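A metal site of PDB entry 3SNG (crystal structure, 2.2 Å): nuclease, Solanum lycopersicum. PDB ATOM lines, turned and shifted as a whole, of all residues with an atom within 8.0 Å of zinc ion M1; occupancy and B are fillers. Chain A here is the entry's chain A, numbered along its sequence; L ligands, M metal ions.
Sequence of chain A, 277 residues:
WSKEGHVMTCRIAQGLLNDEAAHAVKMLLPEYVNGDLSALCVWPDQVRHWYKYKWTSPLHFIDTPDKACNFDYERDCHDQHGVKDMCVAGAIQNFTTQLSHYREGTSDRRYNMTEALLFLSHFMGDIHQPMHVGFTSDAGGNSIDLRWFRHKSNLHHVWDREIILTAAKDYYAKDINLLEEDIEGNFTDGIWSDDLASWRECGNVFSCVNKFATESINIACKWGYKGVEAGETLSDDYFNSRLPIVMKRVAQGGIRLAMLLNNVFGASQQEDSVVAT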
ATOM      1  N   TRP A   1      31.800   2.627 -27.569  1.00  0.00           N
ATOM      2  CA  TRP A   1      31.501   3.286 -28.840  1.00  0.00           C
ATOM      3  C   TRP A   1      30.488   2.479 -29.647  1.00  0.00           C
ATOM      4  O   TRP A   1      30.332   1.260 -29.444  1.00  0.00           O
ATOM      5  CB  TRP A   1      32.750   3.392 -29.708  1.00  0.00           C
ATOM      6  CG  TRP A   1      33.926   4.029 -29.104  1.00  0.00           C
ATOM      7  CD1 TRP A   1      35.028   3.416 -28.689  1.00  0.00           C
ATOM      8  CD2 TRP A   1      34.161   5.444 -28.925  1.00  0.00           C
ATOM      9  NE1 TRP A   1      35.935   4.316 -28.224  1.00  0.00           N
ATOM     10  CE2 TRP A   1      35.427   5.584 -28.358  1.00  0.00           C
ATOM     11  CE3 TRP A   1      33.414   6.594 -29.177  1.00  0.00           C
ATOM     12  CZ2 TRP A   1      35.987   6.817 -28.032  1.00  0.00           C
ATOM     13  CZ3 TRP A   1      33.961   7.835 -28.859  1.00  0.00           C
ATOM     14  CH2 TRP A   1      35.233   7.930 -28.287  1.00  0.00           C
ATOM     15  N   SER A   2      29.841   3.162 -30.566  1.00  0.00           N
ATOM     16  CA  SER A   2      29.124   2.484 -31.662  1.00  0.00           C
ATOM     17  C   SER A   2      30.154   2.112 -32.726  1.00  0.00           C
ATOM     18  O   SER A   2      31.373   2.224 -32.515  1.00  0.00           O
ATOM     19  CB  SER A   2      28.053   3.391 -32.246  1.00  0.00           C
ATOM     20  OG  SER A   2      27.155   3.795 -31.239  1.00  0.00           O
ATOM     21  N   HIS A   6      34.815   2.038 -32.786  1.00  0.00           N
ATOM     22  CA  HIS A   6      35.510   0.742 -32.738  1.00  0.00           C
ATOM     23  C   HIS A   6      36.322   0.480 -33.988  1.00  0.00           C
ATOM     24  O   HIS A   6      37.491   0.035 -33.917  1.00  0.00           O
ATOM     25  CB  HIS A   6      34.484  -0.368 -32.483  1.00  0.00           C
ATOM     26  CG  HIS A   6      34.006  -0.379 -31.059  1.00  0.00           C
ATOM     27  ND1 HIS A   6      34.855  -0.597 -30.006  1.00  0.00           N
ATOM     28  CD2 HIS A   6      32.780  -0.187 -30.524  1.00  0.00           C
ATOM     29  CE1 HIS A   6      34.178  -0.534 -28.877  1.00  0.00           C
ATOM     30  NE2 HIS A   6      32.922  -0.255 -29.153  1.00  0.00           N
ATOM     31  N   ASP A  45      29.464  -6.162 -29.590  1.00  0.00           N
ATOM     32  CA  ASP A  45      28.178  -5.499 -29.524  1.00  0.00           C
ATOM     33  C   ASP A  45      27.016  -6.293 -30.169  1.00  0.00           C
ATOM     34  O   ASP A  45      25.837  -6.070 -29.859  1.00  0.00           O
ATOM     35  CB  ASP A  45      28.279  -4.070 -30.101  1.00  0.00           C
ATOM     36  CG  ASP A  45      28.858  -3.058 -29.067  1.00  0.00           C
ATOM     37  OD1 ASP A  45      28.941  -3.437 -27.862  1.00  0.00           O
ATOM     38  OD2 ASP A  45      29.216  -1.920 -29.438  1.00  0.00           O
ATOM     39  N   ARG A  48      26.576  -9.543 -27.489  1.00  0.00           N
ATOM     40  CA  ARG A  48      26.132  -9.285 -26.123  1.00  0.00           C
ATOM     41  C   ARG A  48      24.629  -9.561 -25.911  1.00  0.00           C
ATOM     42  O   ARG A  48      24.175  -9.778 -24.792  1.00  0.00           O
ATOM     43  CB  ARG A  48      26.417  -7.853 -25.700  1.00  0.00           C
ATOM     44  CG  ARG A  48      25.590  -6.822 -26.400  1.00  0.00           C
ATOM     45  CD  ARG A  48      26.099  -5.420 -26.192  1.00  0.00           C
ATOM     46  NE  ARG A  48      25.937  -4.936 -24.830  1.00  0.00           N
ATOM     47  CZ  ARG A  48      26.364  -3.742 -24.400  1.00  0.00           C
ATOM     48  NH1 ARG A  48      26.958  -2.900 -25.237  1.00  0.00           N
ATOM     49  NH2 ARG A  48      26.167  -3.364 -23.138  1.00  0.00           N
ATOM     50  N   HIS A  60      31.061  -4.255 -20.925  1.00  0.00           N
ATOM     51  CA  HIS A  60      31.280  -3.100 -21.824  1.00  0.00           C
ATOM     52  C   HIS A  60      31.489  -1.747 -21.125  1.00  0.00           C
ATOM     53  O   HIS A  60      31.854  -0.734 -21.788  1.00  0.00           O
ATOM     54  CB  HIS A  60      30.109  -2.964 -22.802  1.00  0.00           C
ATOM     55  CG  HIS A  60      30.025  -4.066 -23.796  1.00  0.00           C
ATOM     56  ND1 HIS A  60      30.344  -3.896 -25.128  1.00  0.00           N
ATOM     57  CD2 HIS A  60      29.717  -5.366 -23.635  1.00  0.00           C
ATOM     58  CE1 HIS A  60      30.201  -5.053 -25.748  1.00  0.00           C
ATOM     59  NE2 HIS A  60      29.826  -5.970 -24.859  1.00  0.00           N
ATOM     60  N   PHE A  61      31.268  -1.691 -19.811  1.00  0.00           N
ATOM     61  CA  PHE A  61      31.212  -0.407 -19.121  1.00  0.00           C
ATOM     62  C   PHE A  61      31.617  -0.532 -17.660  1.00  0.00           C
ATOM     63  O   PHE A  61      31.931  -1.599 -17.186  1.00  0.00           O
ATOM     64  CB  PHE A  61      29.804   0.202 -19.220  1.00  0.00           C
ATOM     65  CG  PHE A  61      28.716  -0.674 -18.641  1.00  0.00           C
ATOM     66  CD1 PHE A  61      28.458  -0.669 -17.284  1.00  0.00           C
ATOM     67  CD2 PHE A  61      27.955  -1.476 -19.451  1.00  0.00           C
ATOM     68  CE1 PHE A  61      27.512  -1.498 -16.737  1.00  0.00           C
ATOM     69  CE2 PHE A  61      26.973  -2.301 -18.905  1.00  0.00           C
ATOM     70  CZ  PHE A  61      26.743  -2.296 -17.542  1.00  0.00           C
ATOM     71  N   HIS A 122      37.715  -4.678 -28.745  1.00  0.00           N
ATOM     72  CA  HIS A 122      36.509  -3.920 -28.514  1.00  0.00           C
ATOM     73  C   HIS A 122      36.541  -3.220 -27.150  1.00  0.00           C
ATOM     74  O   HIS A 122      36.234  -2.036 -27.041  1.00  0.00           O
ATOM     75  CB  HIS A 122      35.311  -4.860 -28.586  1.00  0.00           C
ATOM     76  CG  HIS A 122      33.989  -4.172 -28.431  1.00  0.00           C
ATOM     77  ND1 HIS A 122      33.245  -3.756 -29.509  1.00  0.00           N
ATOM     78  CD2 HIS A 122      33.281  -3.834 -27.324  1.00  0.00           C
ATOM     79  CE1 HIS A 122      32.139  -3.166 -29.075  1.00  0.00           C
ATOM     80  NE2 HIS A 122      32.138  -3.188 -27.751  1.00  0.00           N
ATOM     81  N   ASP A 126      35.948   0.524 -25.609  1.00  0.00           N
ATOM     82  CA  ASP A 126      34.931   0.905 -24.659  1.00  0.00           C
ATOM     83  C   ASP A 126      35.496   1.650 -23.428  1.00  0.00           C
ATOM     84  O   ASP A 126      34.902   2.630 -22.998  1.00  0.00           O
ATOM     85  CB  ASP A 126      34.054  -0.306 -24.236  1.00  0.00           C
ATOM     86  CG  ASP A 126      32.947  -0.625 -25.265  1.00  0.00           C
ATOM     87  OD1 ASP A 126      32.748   0.177 -26.159  1.00  0.00           O
ATOM     88  OD2 ASP A 126      32.208  -1.618 -25.130  1.00  0.00           O
ATOM     89  N   GLN A 129      35.858   5.270 -24.080  1.00  0.00           N
ATOM     90  CA  GLN A 129      34.655   6.087 -24.321  1.00  0.00           C
ATOM     91  C   GLN A 129      34.207   6.636 -22.965  1.00  0.00           C
ATOM     92  O   GLN A 129      33.758   5.878 -22.099  1.00  0.00           O
ATOM     93  CB  GLN A 129      33.532   5.243 -24.944  1.00  0.00           C
ATOM     94  CG  GLN A 129      32.534   6.035 -25.866  1.00  0.00           C
ATOM     95  CD  GLN A 129      31.553   6.933 -25.109  1.00  0.00           C
ATOM     96  OE1 GLN A 129      31.988   7.792 -24.323  1.00  0.00           O
ATOM     97  NE2 GLN A 129      30.239   6.726 -25.318  1.00  0.00           N
ATOM     98  N   MET A 131      31.643   8.080 -21.589  1.00  0.00           N
ATOM     99  CA  MET A 131      30.337   7.682 -21.025  1.00  0.00           C
ATOM    100  C   MET A 131      30.175   6.194 -20.760  1.00  0.00           C
ATOM    101  O   MET A 131      29.189   5.810 -20.135  1.00  0.00           O
ATOM    102  CB  MET A 131      29.183   8.261 -21.844  1.00  0.00           C
ATOM    103  CG  MET A 131      29.389   9.739 -22.155  1.00  0.00           C
ATOM    104  SD  MET A 131      29.583  10.752 -20.642  1.00  0.00           S
ATOM    105  CE  MET A 131      28.027  10.401 -19.879  1.00  0.00           C
ATOM    106  N   HIS A 132      31.158   5.373 -21.150  1.00  0.00           N
ATOM    107  CA  HIS A 132      31.226   3.978 -20.677  1.00  0.00           C
ATOM    108  C   HIS A 132      31.766   3.830 -19.246  1.00  0.00           C
ATOM    109  O   HIS A 132      31.742   2.721 -18.693  1.00  0.00           O
ATOM    110  CB  HIS A 132      32.050   3.118 -21.647  1.00  0.00           C
ATOM    111  CG  HIS A 132      31.266   2.682 -22.843  1.00  0.00           C
ATOM    112  ND1 HIS A 132      31.019   1.361 -23.119  1.00  0.00           N
ATOM    113  CD2 HIS A 132      30.588   3.397 -23.754  1.00  0.00           C
ATOM    114  CE1 HIS A 132      30.246   1.279 -24.202  1.00  0.00           C
ATOM    115  NE2 HIS A 132      29.984   2.495 -24.601  1.00  0.00           N
ATOM    116  N   ALA A 139      22.839   5.207 -16.118  1.00  0.00           N
ATOM    117  CA  ALA A 139      23.484   4.272 -17.054  1.00  0.00           C
ATOM    118  C   ALA A 139      24.445   4.957 -18.015  1.00  0.00           C
ATOM    119  O   ALA A 139      24.341   4.818 -19.237  1.00  0.00           O
ATOM    120  CB  ALA A 139      22.418   3.460 -17.841  1.00  0.00           C
ATOM    121  N   GLY A 140      25.401   5.703 -17.467  1.00  0.00           N
ATOM    122  CA  GLY A 140      26.407   6.346 -18.318  1.00  0.00           C
ATOM    123  C   GLY A 140      25.777   7.287 -19.333  1.00  0.00           C
ATOM    124  O   GLY A 140      26.263   7.440 -20.473  1.00  0.00           O
ATOM    125  N   ASN A 142      22.785   6.967 -20.709  1.00  0.00           N
ATOM    126  CA  ASN A 142      21.751   6.319 -21.512  1.00  0.00           C
ATOM    127  C   ASN A 142      20.347   6.737 -21.103  1.00  0.00           C
ATOM    128  O   ASN A 142      19.426   6.666 -21.912  1.00  0.00           O
ATOM    129  CB  ASN A 142      21.814   4.803 -21.420  1.00  0.00           C
ATOM    130  CG  ASN A 142      22.836   4.196 -22.368  1.00  0.00           C
ATOM    131  OD1 ASN A 142      22.632   4.187 -23.589  1.00  0.00           O
ATOM    132  ND2 ASN A 142      23.942   3.674 -21.807  1.00  0.00           N
ATOM    133  N   ASN A 154      20.270  10.462 -26.818  1.00  0.00           N
ATOM    134  CA  ASN A 154      20.606  10.483 -25.404  1.00  0.00           C
ATOM    135  C   ASN A 154      22.076  10.794 -25.227  1.00  0.00           C
ATOM    136  O   ASN A 154      22.860  10.718 -26.185  1.00  0.00           O
ATOM    137  CB  ASN A 154      20.160   9.198 -24.697  1.00  0.00           C
ATOM    138  CG  ASN A 154      21.004   7.989 -25.089  1.00  0.00           C
ATOM    139  OD1 ASN A 154      22.214   7.937 -24.781  1.00  0.00           O
ATOM    140  ND2 ASN A 154      20.365   7.026 -25.774  1.00  0.00           N
ATOM    141  N   HIS A 156      24.597   9.347 -23.671  1.00  0.00           N
ATOM    142  CA  HIS A 156      25.512   8.221 -24.011  1.00  0.00           C
ATOM    143  C   HIS A 156      25.765   8.116 -25.509  1.00  0.00           C
ATOM    144  O   HIS A 156      26.929   8.023 -25.974  1.00  0.00           O
ATOM    145  CB  HIS A 156      24.961   6.931 -23.482  1.00  0.00           C
ATOM    146  CG  HIS A 156      25.929   5.777 -23.555  1.00  0.00           C
ATOM    147  ND1 HIS A 156      26.704   5.386 -22.489  1.00  0.00           N
ATOM    148  CD2 HIS A 156      26.216   4.918 -24.567  1.00  0.00           C
ATOM    149  CE1 HIS A 156      27.425   4.329 -22.830  1.00  0.00           C
ATOM    150  NE2 HIS A 156      27.161   4.032 -24.087  1.00  0.00           N
ATOM    151  N   HIS A 157      24.669   8.193 -26.265  1.00  0.00           N
ATOM    152  CA  HIS A 157      24.719   8.049 -27.713  1.00  0.00           C
ATOM    153  C   HIS A 157      25.410   9.182 -28.389  1.00  0.00           C
ATOM    154  O   HIS A 157      26.006   9.017 -29.467  1.00  0.00           O
ATOM    155  CB  HIS A 157      23.312   7.868 -28.295  1.00  0.00           C
ATOM    156  CG  HIS A 157      23.311   7.195 -29.629  1.00  0.00           C
ATOM    157  ND1 HIS A 157      23.766   5.904 -29.805  1.00  0.00           N
ATOM    158  CD2 HIS A 157      22.968   7.635 -30.859  1.00  0.00           C
ATOM    159  CE1 HIS A 157      23.669   5.579 -31.075  1.00  0.00           C
ATOM    160  NE2 HIS A 157      23.187   6.606 -31.738  1.00  0.00           N
ATOM    161  N   TRP A 159      28.041  10.526 -27.339  1.00  0.00           N
ATOM    162  CA  TRP A 159      29.472  10.198 -27.241  1.00  0.00           C
ATOM    163  C   TRP A 159      29.799   8.895 -28.008  1.00  0.00           C
ATOM    164  O   TRP A 159      30.846   8.792 -28.623  1.00  0.00           O
ATOM    165  CB  TRP A 159      29.886  10.129 -25.746  1.00  0.00           C
ATOM    166  CG  TRP A 159      30.052  11.517 -25.170  1.00  0.00           C
ATOM    167  CD1 TRP A 159      29.045  12.341 -24.761  1.00  0.00           C
ATOM    168  CD2 TRP A 159      31.275  12.234 -24.959  1.00  0.00           C
ATOM    169  NE1 TRP A 159      29.564  13.540 -24.326  1.00  0.00           N
ATOM    170  CE2 TRP A 159      30.926  13.512 -24.442  1.00  0.00           C
ATOM    171  CE3 TRP A 159      32.628  11.945 -25.153  1.00  0.00           C
ATOM    172  CZ2 TRP A 159      31.869  14.476 -24.098  1.00  0.00           C
ATOM    173  CZ3 TRP A 159      33.580  12.896 -24.825  1.00  0.00           C
ATOM    174  CH2 TRP A 159      33.194  14.162 -24.298  1.00  0.00           C
ATOM    175  N   ASP A 160      28.903   7.913 -27.958  1.00  0.00           N
ATOM    176  CA  ASP A 160      29.118   6.653 -28.696  1.00  0.00           C
ATOM    177  C   ASP A 160      29.165   6.878 -30.197  1.00  0.00           C
ATOM    178  O   ASP A 160      29.906   6.190 -30.892  1.00  0.00           O
ATOM    179  CB  ASP A 160      28.000   5.653 -28.451  1.00  0.00           C
ATOM    180  CG  ASP A 160      28.290   4.645 -27.340  1.00  0.00           C
ATOM    181  OD1 ASP A 160      29.359   4.603 -26.722  1.00  0.00           O
ATOM    182  OD2 ASP A 160      27.411   3.855 -27.096  1.00  0.00           O
ATOM    183  N   ARG A 161      28.381   7.840 -30.699  1.00  0.00           N
ATOM    184  CA  ARG A 161      28.167   7.976 -32.143  1.00  0.00           C
ATOM    185  C   ARG A 161      27.899   9.381 -32.751  1.00  0.00           C
ATOM    186  O   ARG A 161      28.431   9.670 -33.818  1.00  0.00           O
ATOM    187  CB  ARG A 161      27.021   7.040 -32.557  1.00  0.00           C
ATOM    188  CG  ARG A 161      27.084   6.740 -34.004  1.00  0.00           C
ATOM    189  CD  ARG A 161      26.036   5.777 -34.443  1.00  0.00           C
ATOM    190  NE  ARG A 161      26.484   5.129 -35.675  1.00  0.00           N
ATOM    191  CZ  ARG A 161      25.674   4.635 -36.608  1.00  0.00           C
ATOM    192  NH1 ARG A 161      24.362   4.732 -36.486  1.00  0.00           N
ATOM    193  NH2 ARG A 161      26.190   4.050 -37.690  1.00  0.00           N
HETATM  194  S1  LIG L   1      27.043   0.671 -23.017  1.00  0.00           S
HETATM  195  O1  LIG L   1      27.124   1.182 -24.416  1.00  0.00           O
HETATM  196  O2  LIG L   1      28.005   1.331 -22.131  1.00  0.00           O
HETATM  197  O3  LIG L   1      27.253  -0.750 -23.030  1.00  0.00           O
HETATM  198  O4  LIG L   1      25.719   1.057 -22.531  1.00  0.00           O
HETATM  199 ZN    ZN M   1      28.029   2.696 -25.448  1.00  0.00          ZN
HETATM  200 ZN    ZN M   2      31.559   0.502 -27.859  1.00  0.00          ZN
HETATM  201 ZN    ZN M   3      30.877  -2.369 -26.377  1.00  0.00          ZN
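OD1 of Asp 160 lies close to N of Trp 1 (3.3 Å). A ring nitrogen (ND1) of His 156 lies within hydrogen-bond range of the backbone carbonyl oxygen of Gly 140 (2.9 Å). N of His 156 is in hydrogen-bond range of OD1 of Asn 154, 3.0 Å away. A ring nitrogen (ND1) of His 132 lies within hydrogen-bond range of the backbone carbonyl oxygen of His 60, 2.6 Å away. ND1 of His 156 lies within hydrogen-bond range of ND2 of Asn 142 (3.3 Å). ND1 of His 156 lies within hydrogen-bond range of O of Met 131 (3.4 Å). O of Asp 160 lies within hydrogen-bond range of N of Ser 2 (3.0 Å). The side-chain carboxylate (OD1) of Asp 160 lies within hydrogen-bond range of the side-chain amide nitrogen (NE2) of Gln 129 (2.7 Å).
Of the 21 residues printed, 3 come within 4 Å of zinc ion M1.
Zinc ion M1 is bound by an oxygen (O1) of the ligand (2.0 Å), a ring nitrogen (NE2) of His 156 (2.1 Å), the side-chain carboxylate of Asp 160 (2.1 Å) and a ring nitrogen (NE2) of His 132 (2.1 Å). Zinc ion M1 has four donor atoms within binding distance. Slightly farther from zinc ion M1 lies the side-chain carboxylate (OD1) of Asp 160 (2.7 Å).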
